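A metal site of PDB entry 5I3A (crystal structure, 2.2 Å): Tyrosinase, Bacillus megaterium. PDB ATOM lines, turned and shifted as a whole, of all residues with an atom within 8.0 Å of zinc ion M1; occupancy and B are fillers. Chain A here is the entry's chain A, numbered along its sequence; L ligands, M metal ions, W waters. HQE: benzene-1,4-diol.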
ATOM      1  N   HIS A  39       0.245   2.053  29.230  1.00  0.00           N
ATOM      2  CA  HIS A  39      -0.317   2.845  28.146  1.00  0.00           C
ATOM      3  C   HIS A  39      -1.088   1.984  27.155  1.00  0.00           C
ATOM      4  O   HIS A  39      -2.215   2.306  26.781  1.00  0.00           O
ATOM      5  CB  HIS A  39       0.802   3.598  27.420  1.00  0.00           C
ATOM      6  CG  HIS A  39       0.324   4.361  26.228  1.00  0.00           C
ATOM      7  ND1 HIS A  39      -0.283   5.588  26.328  1.00  0.00           N
ATOM      8  CD2 HIS A  39       0.370   4.068  24.908  1.00  0.00           C
ATOM      9  CE1 HIS A  39      -0.598   6.028  25.128  1.00  0.00           C
ATOM     10  NE2 HIS A  39      -0.212   5.120  24.235  1.00  0.00           N
ATOM     11  N   ALA A  56      -7.384   6.127  28.386  1.00  0.00           N
ATOM     12  CA  ALA A  56      -6.318   7.110  28.230  1.00  0.00           C
ATOM     13  C   ALA A  56      -6.512   8.056  27.047  1.00  0.00           C
ATOM     14  O   ALA A  56      -5.830   9.078  26.955  1.00  0.00           O
ATOM     15  CB  ALA A  56      -4.982   6.406  28.114  1.00  0.00           C
ATOM     16  N   HIS A  57      -7.431   7.729  26.140  1.00  0.00           N
ATOM     17  CA  HIS A  57      -7.625   8.541  24.936  1.00  0.00           C
ATOM     18  C   HIS A  57      -9.081   8.695  24.525  1.00  0.00           C
ATOM     19  O   HIS A  57      -9.951   7.982  25.024  1.00  0.00           O
ATOM     20  CB  HIS A  57      -6.861   7.936  23.744  1.00  0.00           C
ATOM     21  CG  HIS A  57      -5.469   7.498  24.065  1.00  0.00           C
ATOM     22  ND1 HIS A  57      -5.181   6.248  24.580  1.00  0.00           N
ATOM     23  CD2 HIS A  57      -4.275   8.131  23.933  1.00  0.00           C
ATOM     24  CE1 HIS A  57      -3.872   6.144  24.754  1.00  0.00           C
ATOM     25  NE2 HIS A  57      -3.303   7.268  24.367  1.00  0.00           N
ATOM     26  N   PHE A  62      -8.391  11.687  28.997  1.00  0.00           N
ATOM     27  CA  PHE A  62      -7.132  11.846  28.266  1.00  0.00           C
ATOM     28  C   PHE A  62      -6.072  12.670  29.000  1.00  0.00           C
ATOM     29  O   PHE A  62      -4.951  12.202  29.196  1.00  0.00           O
ATOM     30  CB  PHE A  62      -7.400  12.500  26.905  1.00  0.00           C
ATOM     31  CG  PHE A  62      -6.150  12.911  26.173  1.00  0.00           C
ATOM     32  CD1 PHE A  62      -5.267  11.963  25.696  1.00  0.00           C
ATOM     33  CD2 PHE A  62      -5.860  14.256  25.983  1.00  0.00           C
ATOM     34  CE1 PHE A  62      -4.117  12.342  25.033  1.00  0.00           C
ATOM     35  CE2 PHE A  62      -4.710  14.636  25.321  1.00  0.00           C
ATOM     36  CZ  PHE A  62      -3.836  13.686  24.838  1.00  0.00           C
ATOM     37  N   TRP A  65      -5.281  11.353  32.805  1.00  0.00           N
ATOM     38  CA  TRP A  65      -4.630  10.047  32.734  1.00  0.00           C
ATOM     39  C   TRP A  65      -3.133  10.207  32.484  1.00  0.00           C
ATOM     40  O   TRP A  65      -2.321   9.587  33.166  1.00  0.00           O
ATOM     41  CB  TRP A  65      -5.246   9.190  31.621  1.00  0.00           C
ATOM     42  CG  TRP A  65      -4.798   7.754  31.654  1.00  0.00           C
ATOM     43  CD1 TRP A  65      -5.481   6.694  32.194  1.00  0.00           C
ATOM     44  CD2 TRP A  65      -3.582   7.216  31.122  1.00  0.00           C
ATOM     45  NE1 TRP A  65      -4.763   5.541  32.032  1.00  0.00           N
ATOM     46  CE2 TRP A  65      -3.589   5.831  31.375  1.00  0.00           C
ATOM     47  CE3 TRP A  65      -2.480   7.774  30.451  1.00  0.00           C
ATOM     48  CZ2 TRP A  65      -2.544   4.994  30.987  1.00  0.00           C
ATOM     49  CZ3 TRP A  65      -1.448   6.933  30.067  1.00  0.00           C
ATOM     50  CH2 TRP A  65      -1.490   5.555  30.339  1.00  0.00           C
ATOM     51  N   HIS A  66      -2.786  11.040  31.505  1.00  0.00           N
ATOM     52  CA  HIS A  66      -1.389  11.235  31.151  1.00  0.00           C
ATOM     53  C   HIS A  66      -0.650  12.056  32.194  1.00  0.00           C
ATOM     54  O   HIS A  66       0.563  11.931  32.339  1.00  0.00           O
ATOM     55  CB  HIS A  66      -1.270  11.884  29.773  1.00  0.00           C
ATOM     56  CG  HIS A  66      -1.588  10.956  28.638  1.00  0.00           C
ATOM     57  ND1 HIS A  66      -2.870  10.731  28.194  1.00  0.00           N
ATOM     58  CD2 HIS A  66      -0.784  10.168  27.888  1.00  0.00           C
ATOM     59  CE1 HIS A  66      -2.845   9.861  27.192  1.00  0.00           C
ATOM     60  NE2 HIS A  66      -1.582   9.502  26.994  1.00  0.00           N
ATOM     61  N   GLU A 192      -6.320  17.336  22.340  1.00  0.00           N
ATOM     62  CA  GLU A 192      -6.016  15.950  21.976  1.00  0.00           C
ATOM     63  C   GLU A 192      -5.802  15.858  20.467  1.00  0.00           C
ATOM     64  O   GLU A 192      -4.867  15.206  20.008  1.00  0.00           O
ATOM     65  CB  GLU A 192      -7.126  15.001  22.423  1.00  0.00           C
ATOM     66  CG  GLU A 192      -6.729  13.524  22.326  1.00  0.00           C
ATOM     67  CD  GLU A 192      -7.746  12.595  22.961  1.00  0.00           C
ATOM     68  OE1 GLU A 192      -8.744  13.092  23.523  1.00  0.00           O
ATOM     69  OE2 GLU A 192      -7.529  11.366  22.908  1.00  0.00           O
ATOM     70  N   HIS A 201      -1.890  17.454  19.735  1.00  0.00           N
ATOM     71  CA  HIS A 201      -1.343  16.219  20.319  1.00  0.00           C
ATOM     72  C   HIS A 201      -1.307  15.050  19.350  1.00  0.00           C
ATOM     73  O   HIS A 201      -0.264  14.385  19.213  1.00  0.00           O
ATOM     74  CB  HIS A 201      -2.147  15.829  21.566  1.00  0.00           C
ATOM     75  CG  HIS A 201      -2.022  14.377  21.915  1.00  0.00           C
ATOM     76  ND1 HIS A 201      -2.930  13.426  21.499  1.00  0.00           N
ATOM     77  CD2 HIS A 201      -1.090  13.719  22.640  1.00  0.00           C
ATOM     78  CE1 HIS A 201      -2.569  12.250  21.958  1.00  0.00           C
ATOM     79  NE2 HIS A 201      -1.450  12.389  22.654  1.00  0.00           N
ATOM     80  N   ASN A 202      -2.419  14.780  18.683  1.00  0.00           N
ATOM     81  CA  ASN A 202      -2.481  13.703  17.698  1.00  0.00           C
ATOM     82  C   ASN A 202      -1.515  13.951  16.537  1.00  0.00           C
ATOM     83  O   ASN A 202      -0.923  13.019  15.998  1.00  0.00           O
ATOM     84  CB  ASN A 202      -3.899  13.524  17.149  1.00  0.00           C
ATOM     85  CG  ASN A 202      -4.832  12.881  18.160  1.00  0.00           C
ATOM     86  OD1 ASN A 202      -4.391  12.287  19.148  1.00  0.00           O
ATOM     87  ND2 ASN A 202      -6.134  12.982  17.907  1.00  0.00           N
ATOM     88  N   VAL A 204       1.356  15.660  16.532  1.00  0.00           N
ATOM     89  CA  VAL A 204       2.743  15.457  16.940  1.00  0.00           C
ATOM     90  C   VAL A 204       3.129  13.983  16.863  1.00  0.00           C
ATOM     91  O   VAL A 204       4.198  13.644  16.351  1.00  0.00           O
ATOM     92  CB  VAL A 204       2.985  15.975  18.377  1.00  0.00           C
ATOM     93  CG1 VAL A 204       4.392  15.641  18.832  1.00  0.00           C
ATOM     94  CG2 VAL A 204       2.726  17.471  18.464  1.00  0.00           C
ATOM     95  N   HIS A 205       2.258  13.121  17.369  1.00  0.00           N
ATOM     96  CA  HIS A 205       2.440  11.671  17.261  1.00  0.00           C
ATOM     97  C   HIS A 205       2.664  11.229  15.825  1.00  0.00           C
ATOM     98  O   HIS A 205       3.659  10.551  15.524  1.00  0.00           O
ATOM     99  CB  HIS A 205       1.232  10.931  17.846  1.00  0.00           C
ATOM    100  CG  HIS A 205       1.284  10.752  19.332  1.00  0.00           C
ATOM    101  ND1 HIS A 205       2.054   9.798  19.941  1.00  0.00           N
ATOM    102  CD2 HIS A 205       0.617  11.392  20.327  1.00  0.00           C
ATOM    103  CE1 HIS A 205       1.887   9.859  21.243  1.00  0.00           C
ATOM    104  NE2 HIS A 205       1.023  10.824  21.504  1.00  0.00           N
ATOM    105  N   MET A 212       5.919   6.025  17.604  1.00  0.00           N
ATOM    106  CA  MET A 212       5.240   7.170  18.173  1.00  0.00           C
ATOM    107  C   MET A 212       3.921   7.477  17.451  1.00  0.00           C
ATOM    108  O   MET A 212       3.026   8.108  18.014  1.00  0.00           O
ATOM    109  CB  MET A 212       6.169   8.392  18.113  1.00  0.00           C
ATOM    110  CG  MET A 212       5.652   9.628  18.823  1.00  0.00           C
ATOM    111  SD  MET A 212       5.799   9.529  20.622  1.00  0.00           S
ATOM    112  CE  MET A 212       5.212  11.161  21.050  1.00  0.00           C
ATOM    113  N   VAL A 215      -0.637   4.028  18.673  1.00  0.00           N
ATOM    114  CA  VAL A 215      -1.045   3.992  20.073  1.00  0.00           C
ATOM    115  C   VAL A 215      -0.365   2.893  20.902  1.00  0.00           C
ATOM    116  O   VAL A 215       0.240   3.156  21.906  1.00  0.00           O
ATOM    117  CB  VAL A 215      -2.573   3.922  20.200  1.00  0.00           C
ATOM    118  CG1 VAL A 215      -3.041   3.562  21.602  1.00  0.00           C
ATOM    119  CG2 VAL A 215      -3.222   5.213  19.771  1.00  0.00           C
ATOM    120  N   ALA A 218       3.614   3.672  21.118  1.00  0.00           N
ATOM    121  CA  ALA A 218       4.122   5.041  21.267  1.00  0.00           C
ATOM    122  C   ALA A 218       5.163   5.275  22.385  1.00  0.00           C
ATOM    123  O   ALA A 218       6.160   5.958  22.155  1.00  0.00           O
ATOM    124  CB  ALA A 218       2.952   6.014  21.435  1.00  0.00           C
ATOM    125  N   PRO A 219       4.928   4.744  23.597  1.00  0.00           N
ATOM    126  CA  PRO A 219       5.907   5.057  24.654  1.00  0.00           C
ATOM    127  C   PRO A 219       7.275   4.393  24.485  1.00  0.00           C
ATOM    128  O   PRO A 219       8.165   4.647  25.297  1.00  0.00           O
ATOM    129  CB  PRO A 219       5.229   4.528  25.925  1.00  0.00           C
ATOM    130  CG  PRO A 219       3.775   4.497  25.592  1.00  0.00           C
ATOM    131  CD  PRO A 219       3.740   4.088  24.161  1.00  0.00           C
ATOM    132  N   PHE A 224       8.027  10.515  23.846  1.00  0.00           N
ATOM    133  CA  PHE A 224       6.622  10.413  24.250  1.00  0.00           C
ATOM    134  C   PHE A 224       6.353  11.240  25.493  1.00  0.00           C
ATOM    135  O   PHE A 224       5.396  12.018  25.557  1.00  0.00           O
ATOM    136  CB  PHE A 224       6.238   8.948  24.484  1.00  0.00           C
ATOM    137  CG  PHE A 224       4.804   8.748  24.911  1.00  0.00           C
ATOM    138  CD1 PHE A 224       4.444   8.812  26.251  1.00  0.00           C
ATOM    139  CD2 PHE A 224       3.819   8.493  23.975  1.00  0.00           C
ATOM    140  CE1 PHE A 224       3.128   8.620  26.645  1.00  0.00           C
ATOM    141  CE2 PHE A 224       2.499   8.303  24.355  1.00  0.00           C
ATOM    142  CZ  PHE A 224       2.161   8.373  25.696  1.00  0.00           C
ATOM    143  N   HIS A 227       6.874  14.952  24.845  1.00  0.00           N
ATOM    144  CA  HIS A 227       5.675  15.396  24.133  1.00  0.00           C
ATOM    145  C   HIS A 227       4.536  15.677  25.100  1.00  0.00           C
ATOM    146  O   HIS A 227       3.952  16.763  25.094  1.00  0.00           O
ATOM    147  CB  HIS A 227       5.250  14.341  23.112  1.00  0.00           C
ATOM    148  CG  HIS A 227       3.930  14.611  22.469  1.00  0.00           C
ATOM    149  ND1 HIS A 227       3.418  15.886  22.307  1.00  0.00           N
ATOM    150  CD2 HIS A 227       2.999  13.769  21.951  1.00  0.00           C
ATOM    151  CE1 HIS A 227       2.241  15.814  21.721  1.00  0.00           C
ATOM    152  NE2 HIS A 227       1.962  14.545  21.494  1.00  0.00           N
ATOM    153  N   HIS A 228       4.198  14.689  25.917  1.00  0.00           N
ATOM    154  CA  HIS A 228       3.056  14.804  26.815  1.00  0.00           C
ATOM    155  C   HIS A 228       3.325  15.752  27.993  1.00  0.00           C
ATOM    156  O   HIS A 228       2.383  16.245  28.603  1.00  0.00           O
ATOM    157  CB  HIS A 228       2.640  13.434  27.320  1.00  0.00           C
ATOM    158  CG  HIS A 228       1.685  12.728  26.409  1.00  0.00           C
ATOM    159  ND1 HIS A 228       0.335  12.985  26.417  1.00  0.00           N
ATOM    160  CD2 HIS A 228       1.890  11.792  25.457  1.00  0.00           C
ATOM    161  CE1 HIS A 228      -0.258  12.231  25.509  1.00  0.00           C
ATOM    162  NE2 HIS A 228       0.663  11.509  24.905  1.00  0.00           N
ATOM    163  N   VAL A 231       2.066  18.772  26.481  1.00  0.00           N
ATOM    164  CA  VAL A 231       0.607  18.679  26.506  1.00  0.00           C
ATOM    165  C   VAL A 231       0.124  18.934  27.931  1.00  0.00           C
ATOM    166  O   VAL A 231      -0.837  19.681  28.145  1.00  0.00           O
ATOM    167  CB  VAL A 231       0.113  17.305  26.027  1.00  0.00           C
ATOM    168  CG1 VAL A 231      -1.390  17.189  26.208  1.00  0.00           C
ATOM    169  CG2 VAL A 231       0.503  17.071  24.576  1.00  0.00           C
HETATM  170  C1  HQE L   1      -0.339   7.848  19.963  1.00  0.00           C
HETATM  171  C2  HQE L   1      -0.884   8.856  19.189  1.00  0.00           C
HETATM  172  C3  HQE L   1      -1.978   9.577  19.666  1.00  0.00           C
HETATM  173  O3  HQE L   1      -2.546  10.601  18.887  1.00  0.00           O
HETATM  174  C4  HQE L   1      -2.524   9.262  20.897  1.00  0.00           C
HETATM  175  C5  HQE L   1      -1.976   8.244  21.668  1.00  0.00           C
HETATM  176  C6  HQE L   1      -0.879   7.544  21.200  1.00  0.00           C
HETATM  177  O6  HQE L   1      -0.332   6.513  21.979  1.00  0.00           O
HETATM  178 ZN    ZN M   1      -0.188  10.740  23.296  1.00  0.00          ZN
HETATM  179 ZN    ZN M   2      -1.316   7.467  23.759  1.00  0.00          ZN
HETATM  180  O   HOH W   1      -0.900   9.234  24.539  1.00  0.00           O
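Phe 224 touches zinc ion M1 (CE2 to ZN, 3.8 Å).
A ring nitrogen (NE2) of His 39 lies close to an oxygen (O6) of the ligand.
The side-chain amide oxygen of Asn 202 lies within hydrogen-bond range of an oxygen (O3) of the ligand, at 2.5 Å.
The backbone carbonyl oxygen (O) of Val 215 lies close to an oxygen (O6) of the ligand (3.4 Å).
The backbone carbonyl oxygen (O) of Met 212 lies within hydrogen-bond range of a ring nitrogen (ND1) of His 205 (2.7 Å).
The backbone carbonyl oxygen (O) of His 201 lies within hydrogen-bond range of a ring nitrogen (NE2) of His 227, 3.2 Å away.
A ring nitrogen (ND1) of His 201 is in hydrogen-bond range of the side-chain amide oxygen (OD1) of Asn 202 (3.0 Å).
O of Glu 192 is in hydrogen-bond range of ND1 of His 201.
Zinc ion M1 is bound by a ring nitrogen (NE2) of His 228 (2.0 Å), water W1 (2.1 Å), a ring nitrogen (NE2) of His 205 (2.2 Å) and a ring nitrogen (NE2) of His 201 (2.2 Å).
Zinc ion M1 has four donor atoms within binding distance.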
